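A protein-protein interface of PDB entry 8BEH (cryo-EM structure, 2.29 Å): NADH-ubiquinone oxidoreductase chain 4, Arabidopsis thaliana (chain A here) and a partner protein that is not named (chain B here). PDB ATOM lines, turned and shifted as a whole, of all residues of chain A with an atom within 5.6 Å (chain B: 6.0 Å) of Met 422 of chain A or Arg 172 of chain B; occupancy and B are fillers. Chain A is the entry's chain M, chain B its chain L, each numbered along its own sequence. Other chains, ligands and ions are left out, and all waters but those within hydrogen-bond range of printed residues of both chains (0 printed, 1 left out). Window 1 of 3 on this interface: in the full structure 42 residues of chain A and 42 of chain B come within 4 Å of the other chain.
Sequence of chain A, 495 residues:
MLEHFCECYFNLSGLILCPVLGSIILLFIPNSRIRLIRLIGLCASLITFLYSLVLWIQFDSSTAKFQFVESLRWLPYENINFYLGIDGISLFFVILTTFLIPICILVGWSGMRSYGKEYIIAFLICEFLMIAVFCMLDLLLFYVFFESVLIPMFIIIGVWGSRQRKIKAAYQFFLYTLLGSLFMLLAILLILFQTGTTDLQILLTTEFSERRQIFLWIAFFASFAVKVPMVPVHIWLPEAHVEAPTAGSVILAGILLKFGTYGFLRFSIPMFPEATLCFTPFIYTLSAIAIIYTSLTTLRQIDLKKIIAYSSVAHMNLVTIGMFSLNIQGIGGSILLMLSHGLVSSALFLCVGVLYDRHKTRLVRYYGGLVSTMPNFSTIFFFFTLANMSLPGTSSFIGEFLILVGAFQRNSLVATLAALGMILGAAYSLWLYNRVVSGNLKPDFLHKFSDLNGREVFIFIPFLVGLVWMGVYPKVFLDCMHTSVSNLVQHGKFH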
ATOM      1  N   MET A 389     -18.436   7.964 -24.106  1.00  0.00           N
ATOM      2  CA  MET A 389     -19.224   9.111 -24.660  1.00  0.00           C
ATOM      3  C   MET A 389     -20.731   8.938 -24.342  1.00  0.00           C
ATOM      4  O   MET A 389     -21.491   9.689 -24.870  1.00  0.00           O
ATOM      5  CB  MET A 389     -19.021   9.262 -26.176  1.00  0.00           C
ATOM      6  CG  MET A 389     -17.641   9.269 -26.732  1.00  0.00           C
ATOM      7  SD  MET A 389     -17.625   9.147 -28.556  1.00  0.00           S
ATOM      8  CE  MET A 389     -19.095  10.067 -29.002  1.00  0.00           C
ATOM      9  N   SER A 390     -21.126   7.914 -23.615  1.00  0.00           N
ATOM     10  CA  SER A 390     -22.560   7.616 -23.254  1.00  0.00           C
ATOM     11  C   SER A 390     -23.394   7.310 -24.522  1.00  0.00           C
ATOM     12  O   SER A 390     -24.502   7.777 -24.577  1.00  0.00           O
ATOM     13  CB  SER A 390     -23.168   8.671 -22.366  1.00  0.00           C
ATOM     14  OG  SER A 390     -22.665   8.603 -21.056  1.00  0.00           O
ATOM     15  N   LEU A 391     -22.777   6.740 -25.543  1.00  0.00           N
ATOM     16  CA  LEU A 391     -23.486   6.240 -26.732  1.00  0.00           C
ATOM     17  C   LEU A 391     -24.666   5.335 -26.362  1.00  0.00           C
ATOM     18  O   LEU A 391     -24.500   4.353 -25.708  1.00  0.00           O
ATOM     19  CB  LEU A 391     -22.543   5.491 -27.661  1.00  0.00           C
ATOM     20  CG  LEU A 391     -23.132   5.272 -29.054  1.00  0.00           C
ATOM     21  CD1 LEU A 391     -23.054   6.539 -29.885  1.00  0.00           C
ATOM     22  CD2 LEU A 391     -22.509   4.088 -29.772  1.00  0.00           C
ATOM     23  N   PRO A 392     -25.871   5.625 -26.849  1.00  0.00           N
ATOM     24  CA  PRO A 392     -27.002   4.724 -26.593  1.00  0.00           C
ATOM     25  C   PRO A 392     -26.698   3.312 -27.065  1.00  0.00           C
ATOM     26  O   PRO A 392     -26.109   3.099 -28.126  1.00  0.00           O
ATOM     27  CB  PRO A 392     -28.142   5.356 -27.398  1.00  0.00           C
ATOM     28  CG  PRO A 392     -27.786   6.800 -27.457  1.00  0.00           C
ATOM     29  CD  PRO A 392     -26.286   6.851 -27.545  1.00  0.00           C
ATOM     30  N   GLU A 400     -26.698   8.064 -17.549  1.00  0.00           N
ATOM     31  CA  GLU A 400     -26.595   9.468 -17.929  1.00  0.00           C
ATOM     32  C   GLU A 400     -27.965  10.065 -18.226  1.00  0.00           C
ATOM     33  O   GLU A 400     -28.317  11.139 -17.716  1.00  0.00           O
ATOM     34  CB  GLU A 400     -25.667   9.611 -19.132  1.00  0.00           C
ATOM     35  CG  GLU A 400     -25.256  11.030 -19.413  1.00  0.00           C
ATOM     36  CD  GLU A 400     -25.656  11.484 -20.801  1.00  0.00           C
ATOM     37  OE1 GLU A 400     -26.380  10.736 -21.491  1.00  0.00           O
ATOM     38  OE2 GLU A 400     -25.247  12.588 -21.202  1.00  0.00           O
ATOM     39  N   LEU A 404     -30.226  12.890 -16.235  1.00  0.00           N
ATOM     40  CA  LEU A 404     -30.750  14.099 -16.868  1.00  0.00           C
ATOM     41  C   LEU A 404     -32.266  14.201 -16.689  1.00  0.00           C
ATOM     42  O   LEU A 404     -32.795  15.294 -16.461  1.00  0.00           O
ATOM     43  CB  LEU A 404     -30.360  14.140 -18.345  1.00  0.00           C
ATOM     44  CG  LEU A 404     -28.869  14.316 -18.659  1.00  0.00           C
ATOM     45  CD1 LEU A 404     -28.598  14.233 -20.151  1.00  0.00           C
ATOM     46  CD2 LEU A 404     -28.322  15.622 -18.089  1.00  0.00           C
ATOM     47  N   ALA A 418     -25.665  20.254 -17.342  1.00  0.00           N
ATOM     48  CA  ALA A 418     -25.226  18.835 -17.301  1.00  0.00           C
ATOM     49  C   ALA A 418     -25.294  18.139 -18.671  1.00  0.00           C
ATOM     50  O   ALA A 418     -24.407  17.407 -18.948  1.00  0.00           O
ATOM     51  CB  ALA A 418     -25.944  18.086 -16.227  1.00  0.00           C
ATOM     52  N   ALA A 419     -26.251  18.484 -19.520  1.00  0.00           N
ATOM     53  CA  ALA A 419     -26.323  17.909 -20.872  1.00  0.00           C
ATOM     54  C   ALA A 419     -25.163  18.431 -21.790  1.00  0.00           C
ATOM     55  O   ALA A 419     -24.917  17.776 -22.738  1.00  0.00           O
ATOM     56  CB  ALA A 419     -27.709  18.080 -21.416  1.00  0.00           C
ATOM     57  N   LEU A 420     -24.532  19.574 -21.494  1.00  0.00           N
ATOM     58  CA  LEU A 420     -23.285  20.039 -22.210  1.00  0.00           C
ATOM     59  C   LEU A 420     -22.193  18.965 -22.201  1.00  0.00           C
ATOM     60  O   LEU A 420     -21.486  18.902 -23.181  1.00  0.00           O
ATOM     61  CB  LEU A 420     -22.748  21.353 -21.645  1.00  0.00           C
ATOM     62  CG  LEU A 420     -23.674  22.548 -21.850  1.00  0.00           C
ATOM     63  CD1 LEU A 420     -23.183  23.770 -21.098  1.00  0.00           C
ATOM     64  CD2 LEU A 420     -23.874  22.843 -23.326  1.00  0.00           C
ATOM     65  N   GLY A 421     -22.117  18.135 -21.156  1.00  0.00           N
ATOM     66  CA  GLY A 421     -21.213  16.977 -21.112  1.00  0.00           C
ATOM     67  C   GLY A 421     -21.297  16.073 -22.330  1.00  0.00           C
ATOM     68  O   GLY A 421     -20.247  15.609 -22.737  1.00  0.00           O
ATOM     69  N   MET A 422     -22.481  15.826 -22.877  1.00  0.00           N
ATOM     70  CA  MET A 422     -22.646  15.091 -24.146  1.00  0.00           C
ATOM     71  C   MET A 422     -21.737  15.696 -25.229  1.00  0.00           C
ATOM     72  O   MET A 422     -21.196  14.951 -25.988  1.00  0.00           O
ATOM     73  CB  MET A 422     -24.105  15.049 -24.623  1.00  0.00           C
ATOM     74  CG  MET A 422     -25.164  14.701 -23.590  1.00  0.00           C
ATOM     75  SD  MET A 422     -26.849  15.247 -24.115  1.00  0.00           S
ATOM     76  CE  MET A 422     -26.986  14.431 -25.703  1.00  0.00           C
ATOM     77  N   ILE A 423     -21.614  16.987 -25.311  1.00  0.00           N
ATOM     78  CA  ILE A 423     -20.794  17.599 -26.377  1.00  0.00           C
ATOM     79  C   ILE A 423     -19.282  17.520 -26.017  1.00  0.00           C
ATOM     80  O   ILE A 423     -18.516  17.133 -26.848  1.00  0.00           O
ATOM     81  CB  ILE A 423     -21.266  19.035 -26.724  1.00  0.00           C
ATOM     82  CG1 ILE A 423     -22.747  19.085 -27.116  1.00  0.00           C
ATOM     83  CG2 ILE A 423     -20.374  19.681 -27.773  1.00  0.00           C
ATOM     84  CD1 ILE A 423     -23.383  20.449 -26.956  1.00  0.00           C
ATOM     85  N   LEU A 424     -18.936  17.831 -24.789  1.00  0.00           N
ATOM     86  CA  LEU A 424     -17.521  17.932 -24.425  1.00  0.00           C
ATOM     87  C   LEU A 424     -16.859  16.555 -24.294  1.00  0.00           C
ATOM     88  O   LEU A 424     -15.724  16.355 -24.758  1.00  0.00           O
ATOM     89  CB  LEU A 424     -17.380  18.749 -23.143  1.00  0.00           C
ATOM     90  CG  LEU A 424     -17.885  20.192 -23.240  1.00  0.00           C
ATOM     91  CD1 LEU A 424     -17.815  20.896 -21.900  1.00  0.00           C
ATOM     92  CD2 LEU A 424     -17.118  20.978 -24.297  1.00  0.00           C
ATOM     93  N   GLY A 425     -17.548  15.599 -23.663  1.00  0.00           N
ATOM     94  CA  GLY A 425     -17.004  14.260 -23.540  1.00  0.00           C
ATOM     95  C   GLY A 425     -16.788  13.593 -24.881  1.00  0.00           C
ATOM     96  O   GLY A 425     -15.768  12.935 -25.098  1.00  0.00           O
ATOM     97  N   ALA A 426     -17.732  13.791 -25.839  1.00  0.00           N
ATOM     98  CA  ALA A 426     -17.537  13.311 -27.218  1.00  0.00           C
ATOM     99  C   ALA A 426     -16.248  13.918 -27.769  1.00  0.00           C
ATOM    100  O   ALA A 426     -15.486  13.213 -28.350  1.00  0.00           O
ATOM    101  CB  ALA A 426     -18.688  13.615 -28.169  1.00  0.00           C
ATOM    102  N   ALA A 427     -16.138  15.203 -27.620  1.00  0.00           N
ATOM    103  CA  ALA A 427     -14.986  15.867 -28.215  1.00  0.00           C
ATOM    104  C   ALA A 427     -13.678  15.235 -27.745  1.00  0.00           C
ATOM    105  O   ALA A 427     -12.860  14.794 -28.564  1.00  0.00           O
ATOM    106  CB  ALA A 427     -15.016  17.361 -27.893  1.00  0.00           C
ATOM    107  N   PHE B 137     -33.862   8.122 -30.518  1.00  0.00           N
ATOM    108  CA  PHE B 137     -32.572   8.685 -30.135  1.00  0.00           C
ATOM    109  C   PHE B 137     -31.446   7.683 -30.363  1.00  0.00           C
ATOM    110  O   PHE B 137     -30.346   8.055 -30.787  1.00  0.00           O
ATOM    111  CB  PHE B 137     -32.623   9.132 -28.675  1.00  0.00           C
ATOM    112  CG  PHE B 137     -31.466   9.980 -28.257  1.00  0.00           C
ATOM    113  CD1 PHE B 137     -31.431  11.326 -28.564  1.00  0.00           C
ATOM    114  CD2 PHE B 137     -30.413   9.433 -27.545  1.00  0.00           C
ATOM    115  CE1 PHE B 137     -30.366  12.112 -28.174  1.00  0.00           C
ATOM    116  CE2 PHE B 137     -29.344  10.215 -27.154  1.00  0.00           C
ATOM    117  CZ  PHE B 137     -29.323  11.556 -27.467  1.00  0.00           C
ATOM    118  N   GLU B 141     -28.256   8.520 -32.772  1.00  0.00           N
ATOM    119  CA  GLU B 141     -26.819   8.407 -32.403  1.00  0.00           C
ATOM    120  C   GLU B 141     -26.141   7.333 -33.263  1.00  0.00           C
ATOM    121  O   GLU B 141     -24.967   7.535 -33.623  1.00  0.00           O
ATOM    122  CB  GLU B 141     -26.668   8.094 -30.916  1.00  0.00           C
ATOM    123  CG  GLU B 141     -27.478   9.020 -30.033  1.00  0.00           C
ATOM    124  CD  GLU B 141     -27.233  10.502 -30.231  1.00  0.00           C
ATOM    125  OE1 GLU B 141     -26.135  10.969 -29.872  1.00  0.00           O
ATOM    126  OE2 GLU B 141     -28.147  11.179 -30.740  1.00  0.00           O
ATOM    127  N   ALA B 167     -18.171  16.456 -38.142  1.00  0.00           N
ATOM    128  CA  ALA B 167     -19.533  15.955 -38.301  1.00  0.00           C
ATOM    129  C   ALA B 167     -20.075  15.430 -36.977  1.00  0.00           C
ATOM    130  O   ALA B 167     -21.201  15.756 -36.580  1.00  0.00           O
ATOM    131  CB  ALA B 167     -19.571  14.867 -39.373  1.00  0.00           C
ATOM    132  N   MET B 168     -19.326  14.549 -36.304  1.00  0.00           N
ATOM    133  CA  MET B 168     -19.759  14.084 -34.955  1.00  0.00           C
ATOM    134  C   MET B 168     -20.061  15.216 -33.958  1.00  0.00           C
ATOM    135  O   MET B 168     -21.071  15.117 -33.319  1.00  0.00           O
ATOM    136  CB  MET B 168     -18.801  13.070 -34.321  1.00  0.00           C
ATOM    137  CG  MET B 168     -19.012  11.665 -34.776  1.00  0.00           C
ATOM    138  SD  MET B 168     -20.223  10.742 -33.804  1.00  0.00           S
ATOM    139  CE  MET B 168     -20.256  11.735 -32.316  1.00  0.00           C
ATOM    140  N   LEU B 169     -19.216  16.222 -33.844  1.00  0.00           N
ATOM    141  CA  LEU B 169     -19.414  17.330 -32.880  1.00  0.00           C
ATOM    142  C   LEU B 169     -20.642  18.206 -33.229  1.00  0.00           C
ATOM    143  O   LEU B 169     -21.350  18.554 -32.344  1.00  0.00           O
ATOM    144  CB  LEU B 169     -18.149  18.178 -32.819  1.00  0.00           C
ATOM    145  CG  LEU B 169     -16.900  17.483 -32.265  1.00  0.00           C
ATOM    146  CD1 LEU B 169     -15.651  18.347 -32.374  1.00  0.00           C
ATOM    147  CD2 LEU B 169     -17.107  17.030 -30.834  1.00  0.00           C
ATOM    148  N   VAL B 170     -20.825  18.549 -34.495  1.00  0.00           N
ATOM    149  CA  VAL B 170     -22.045  19.310 -34.914  1.00  0.00           C
ATOM    150  C   VAL B 170     -23.294  18.479 -34.597  1.00  0.00           C
ATOM    151  O   VAL B 170     -24.160  19.027 -33.979  1.00  0.00           O
ATOM    152  CB  VAL B 170     -21.961  19.838 -36.366  1.00  0.00           C
ATOM    153  CG1 VAL B 170     -23.154  20.702 -36.707  1.00  0.00           C
ATOM    154  CG2 VAL B 170     -20.683  20.624 -36.615  1.00  0.00           C
ATOM    155  N   ASN B 171     -23.270  17.191 -34.892  1.00  0.00           N
ATOM    156  CA  ASN B 171     -24.419  16.293 -34.632  1.00  0.00           C
ATOM    157  C   ASN B 171     -24.679  16.182 -33.126  1.00  0.00           C
ATOM    158  O   ASN B 171     -25.809  16.240 -32.774  1.00  0.00           O
ATOM    159  CB  ASN B 171     -24.337  15.006 -35.462  1.00  0.00           C
ATOM    160  CG  ASN B 171     -24.791  15.311 -36.884  1.00  0.00           C
ATOM    161  OD1 ASN B 171     -25.976  15.532 -37.128  1.00  0.00           O
ATOM    162  ND2 ASN B 171     -23.866  15.418 -37.829  1.00  0.00           N
ATOM    163  N   ARG B 172     -23.615  16.135 -32.304  1.00  0.00           N
ATOM    164  CA  ARG B 172     -23.770  16.130 -30.831  1.00  0.00           C
ATOM    165  C   ARG B 172     -24.472  17.424 -30.363  1.00  0.00           C
ATOM    166  O   ARG B 172     -25.229  17.321 -29.460  1.00  0.00           O
ATOM    167  CB  ARG B 172     -22.445  15.811 -30.111  1.00  0.00           C
ATOM    168  CG  ARG B 172     -22.222  14.328 -29.863  1.00  0.00           C
ATOM    169  CD  ARG B 172     -23.050  13.806 -28.705  1.00  0.00           C
ATOM    170  NE  ARG B 172     -22.903  12.379 -28.488  1.00  0.00           N
ATOM    171  CZ  ARG B 172     -22.325  11.799 -27.438  1.00  0.00           C
ATOM    172  NH1 ARG B 172     -21.809  12.519 -26.460  1.00  0.00           N
ATOM    173  NH2 ARG B 172     -22.257  10.483 -27.372  1.00  0.00           N
ATOM    174  N   VAL B 173     -24.185  18.550 -30.956  1.00  0.00           N
ATOM    175  CA  VAL B 173     -24.880  19.831 -30.594  1.00  0.00           C
ATOM    176  C   VAL B 173     -26.374  19.717 -30.899  1.00  0.00           C
ATOM    177  O   VAL B 173     -27.142  20.132 -30.094  1.00  0.00           O
ATOM    178  CB  VAL B 173     -24.210  21.104 -31.167  1.00  0.00           C
ATOM    179  CG1 VAL B 173     -25.057  22.352 -30.988  1.00  0.00           C
ATOM    180  CG2 VAL B 173     -22.817  21.330 -30.607  1.00  0.00           C
ATOM    181  N   GLY B 174     -26.725  19.037 -31.970  1.00  0.00           N
ATOM    182  CA  GLY B 174     -28.134  18.759 -32.270  1.00  0.00           C
ATOM    183  C   GLY B 174     -28.701  17.755 -31.350  1.00  0.00           C
ATOM    184  O   GLY B 174     -29.788  17.972 -30.889  1.00  0.00           O
ATOM    185  N   ASP B 175     -27.945  16.693 -31.064  1.00  0.00           N
ATOM    186  CA  ASP B 175     -28.376  15.649 -30.110  1.00  0.00           C
ATOM    187  C   ASP B 175     -28.635  16.276 -28.728  1.00  0.00           C
ATOM    188  O   ASP B 175     -29.587  15.865 -28.117  1.00  0.00           O
ATOM    189  CB  ASP B 175     -27.392  14.482 -30.104  1.00  0.00           C
ATOM    190  CG  ASP B 175     -27.043  13.939 -31.474  1.00  0.00           C
ATOM    191  OD1 ASP B 175     -27.793  14.217 -32.423  1.00  0.00           O
ATOM    192  OD2 ASP B 175     -25.992  13.304 -31.590  1.00  0.00           O
ATOM    193  N   PHE B 176     -27.850  17.273 -28.331  1.00  0.00           N
ATOM    194  CA  PHE B 176     -28.065  18.014 -27.070  1.00  0.00           C
ATOM    195  C   PHE B 176     -29.470  18.614 -27.138  1.00  0.00           C
ATOM    196  O   PHE B 176     -30.249  18.410 -26.270  1.00  0.00           O
ATOM    197  CB  PHE B 176     -26.996  19.095 -26.858  1.00  0.00           C
ATOM    198  CG  PHE B 176     -27.274  20.224 -25.909  1.00  0.00           C
ATOM    199  CD1 PHE B 176     -26.994  20.091 -24.560  1.00  0.00           C
ATOM    200  CD2 PHE B 176     -27.720  21.447 -26.377  1.00  0.00           C
ATOM    201  CE1 PHE B 176     -27.209  21.142 -23.688  1.00  0.00           C
ATOM    202  CE2 PHE B 176     -27.930  22.500 -25.504  1.00  0.00           C
ATOM    203  CZ  PHE B 176     -27.671  22.345 -24.163  1.00  0.00           C
ATOM    204  N   GLY B 177     -29.668  19.337 -28.233  1.00  0.00           N
ATOM    205  CA  GLY B 177     -30.996  19.926 -28.362  1.00  0.00           C
ATOM    206  C   GLY B 177     -32.104  18.884 -28.336  1.00  0.00           C
ATOM    207  O   GLY B 177     -33.114  19.039 -27.639  1.00  0.00           O
ATOM    208  N   ALA B 179     -32.091  15.821 -27.042  1.00  0.00           N
ATOM    209  CA  ALA B 179     -32.218  15.207 -25.726  1.00  0.00           C
ATOM    210  C   ALA B 179     -32.939  16.127 -24.751  1.00  0.00           C
ATOM    211  O   ALA B 179     -33.767  15.665 -23.957  1.00  0.00           O
ATOM    212  CB  ALA B 179     -30.839  14.825 -25.188  1.00  0.00           C
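Among the printed residues, merely in contact across the chains: Met 389 of chain A with Met 168 of chain B (3.9 Å), Pro 392 of chain A with Phe 137 of chain B (3.7 Å), Pro 392 of chain A with Glu 141 of chain B (3.4 Å), Ala 419 of chain A with Phe 176 of chain B (3.6 Å), Leu 420 of chain A with Phe 176 of chain B (3.8 Å), Met 422 of chain A with Asp 175 of chain B (3.8 Å), Met 422 of chain A with Phe 176 of chain B (3.97 Å), Met 422 of chain A with Ala 179 of chain B (3.9 Å), Ile 423 of chain A with Arg 172 of chain B (3.8 Å), Ile 423 of chain A with Val 173 of chain B (3.8 Å), Ile 423 of chain A with Phe 176 of chain B (3.9 Å), Ala 426 of chain A with Arg 172 of chain B (3.7 Å) and Ala 427 of chain A with Leu 169 of chain B (3.6 Å).
Of the 16 printed residues of chain A, 8 touch a printed residue of chain B.
Hydrophobic or aromatic side chains of chain A that line the printed part of chain B: Met 389, Pro 392, Ala 419, Leu 420, Met 422, Ile 423, Ala 426 and Ala 427.
Hydrophobic or aromatic side chains of chain B within 4 Å of the printed part of chain A: Phe 137, Met 168, Leu 169, Val 173, Phe 176 and Ala 179.
Among the printed residues, no Asp or Glu carboxylate lies within 4 Å of a Lys or Arg side-chain nitrogen of the other chain.
OE1 of Glu 141 of chain B lies within salt-bridge range of NE of Arg 172 of chain B.
O of Met 389 of chain A sits at hydrogen-bond distance from NH2 of Arg 172 of chain B, 2.7 Å away.
NH1 of Arg 172 of chain B sits at hydrogen-bond distance from O of Met 422 of chain A (2.6 Å).
Gly 421 of chain A touches none of the printed residues of chain B.
Of chain B, only Arg 172, Asp 175, Phe 176 and Ala 179 come within 4 Å of Met 422 of chain A.
Printed residues of chain A within 4 Å of Arg 172 of chain B: Met 389, Met 422, Ile 423 and Ala 426.
Of the printed residues of chain A, Asp 175 of chain B touches Met 422 (3.8 Å).
Printed residues of chain A within 4 Å of Phe 176 of chain B: Ala 419 (3.6 Å), Leu 420 (3.8 Å), Met 422 (3.97 Å) and Ile 423 (3.9 Å).
Printed residues of chain A within 4 Å of Ala 179 of chain B: Met 422 (3.9 Å).
The nearest residue of chain B that does not touch Met 422 of chain A is Phe 137 of chain B (4.1 Å).
The nearest printed residue of chain A that does not touch Val 173 of chain B is Met 422 of chain A (6.8 Å).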
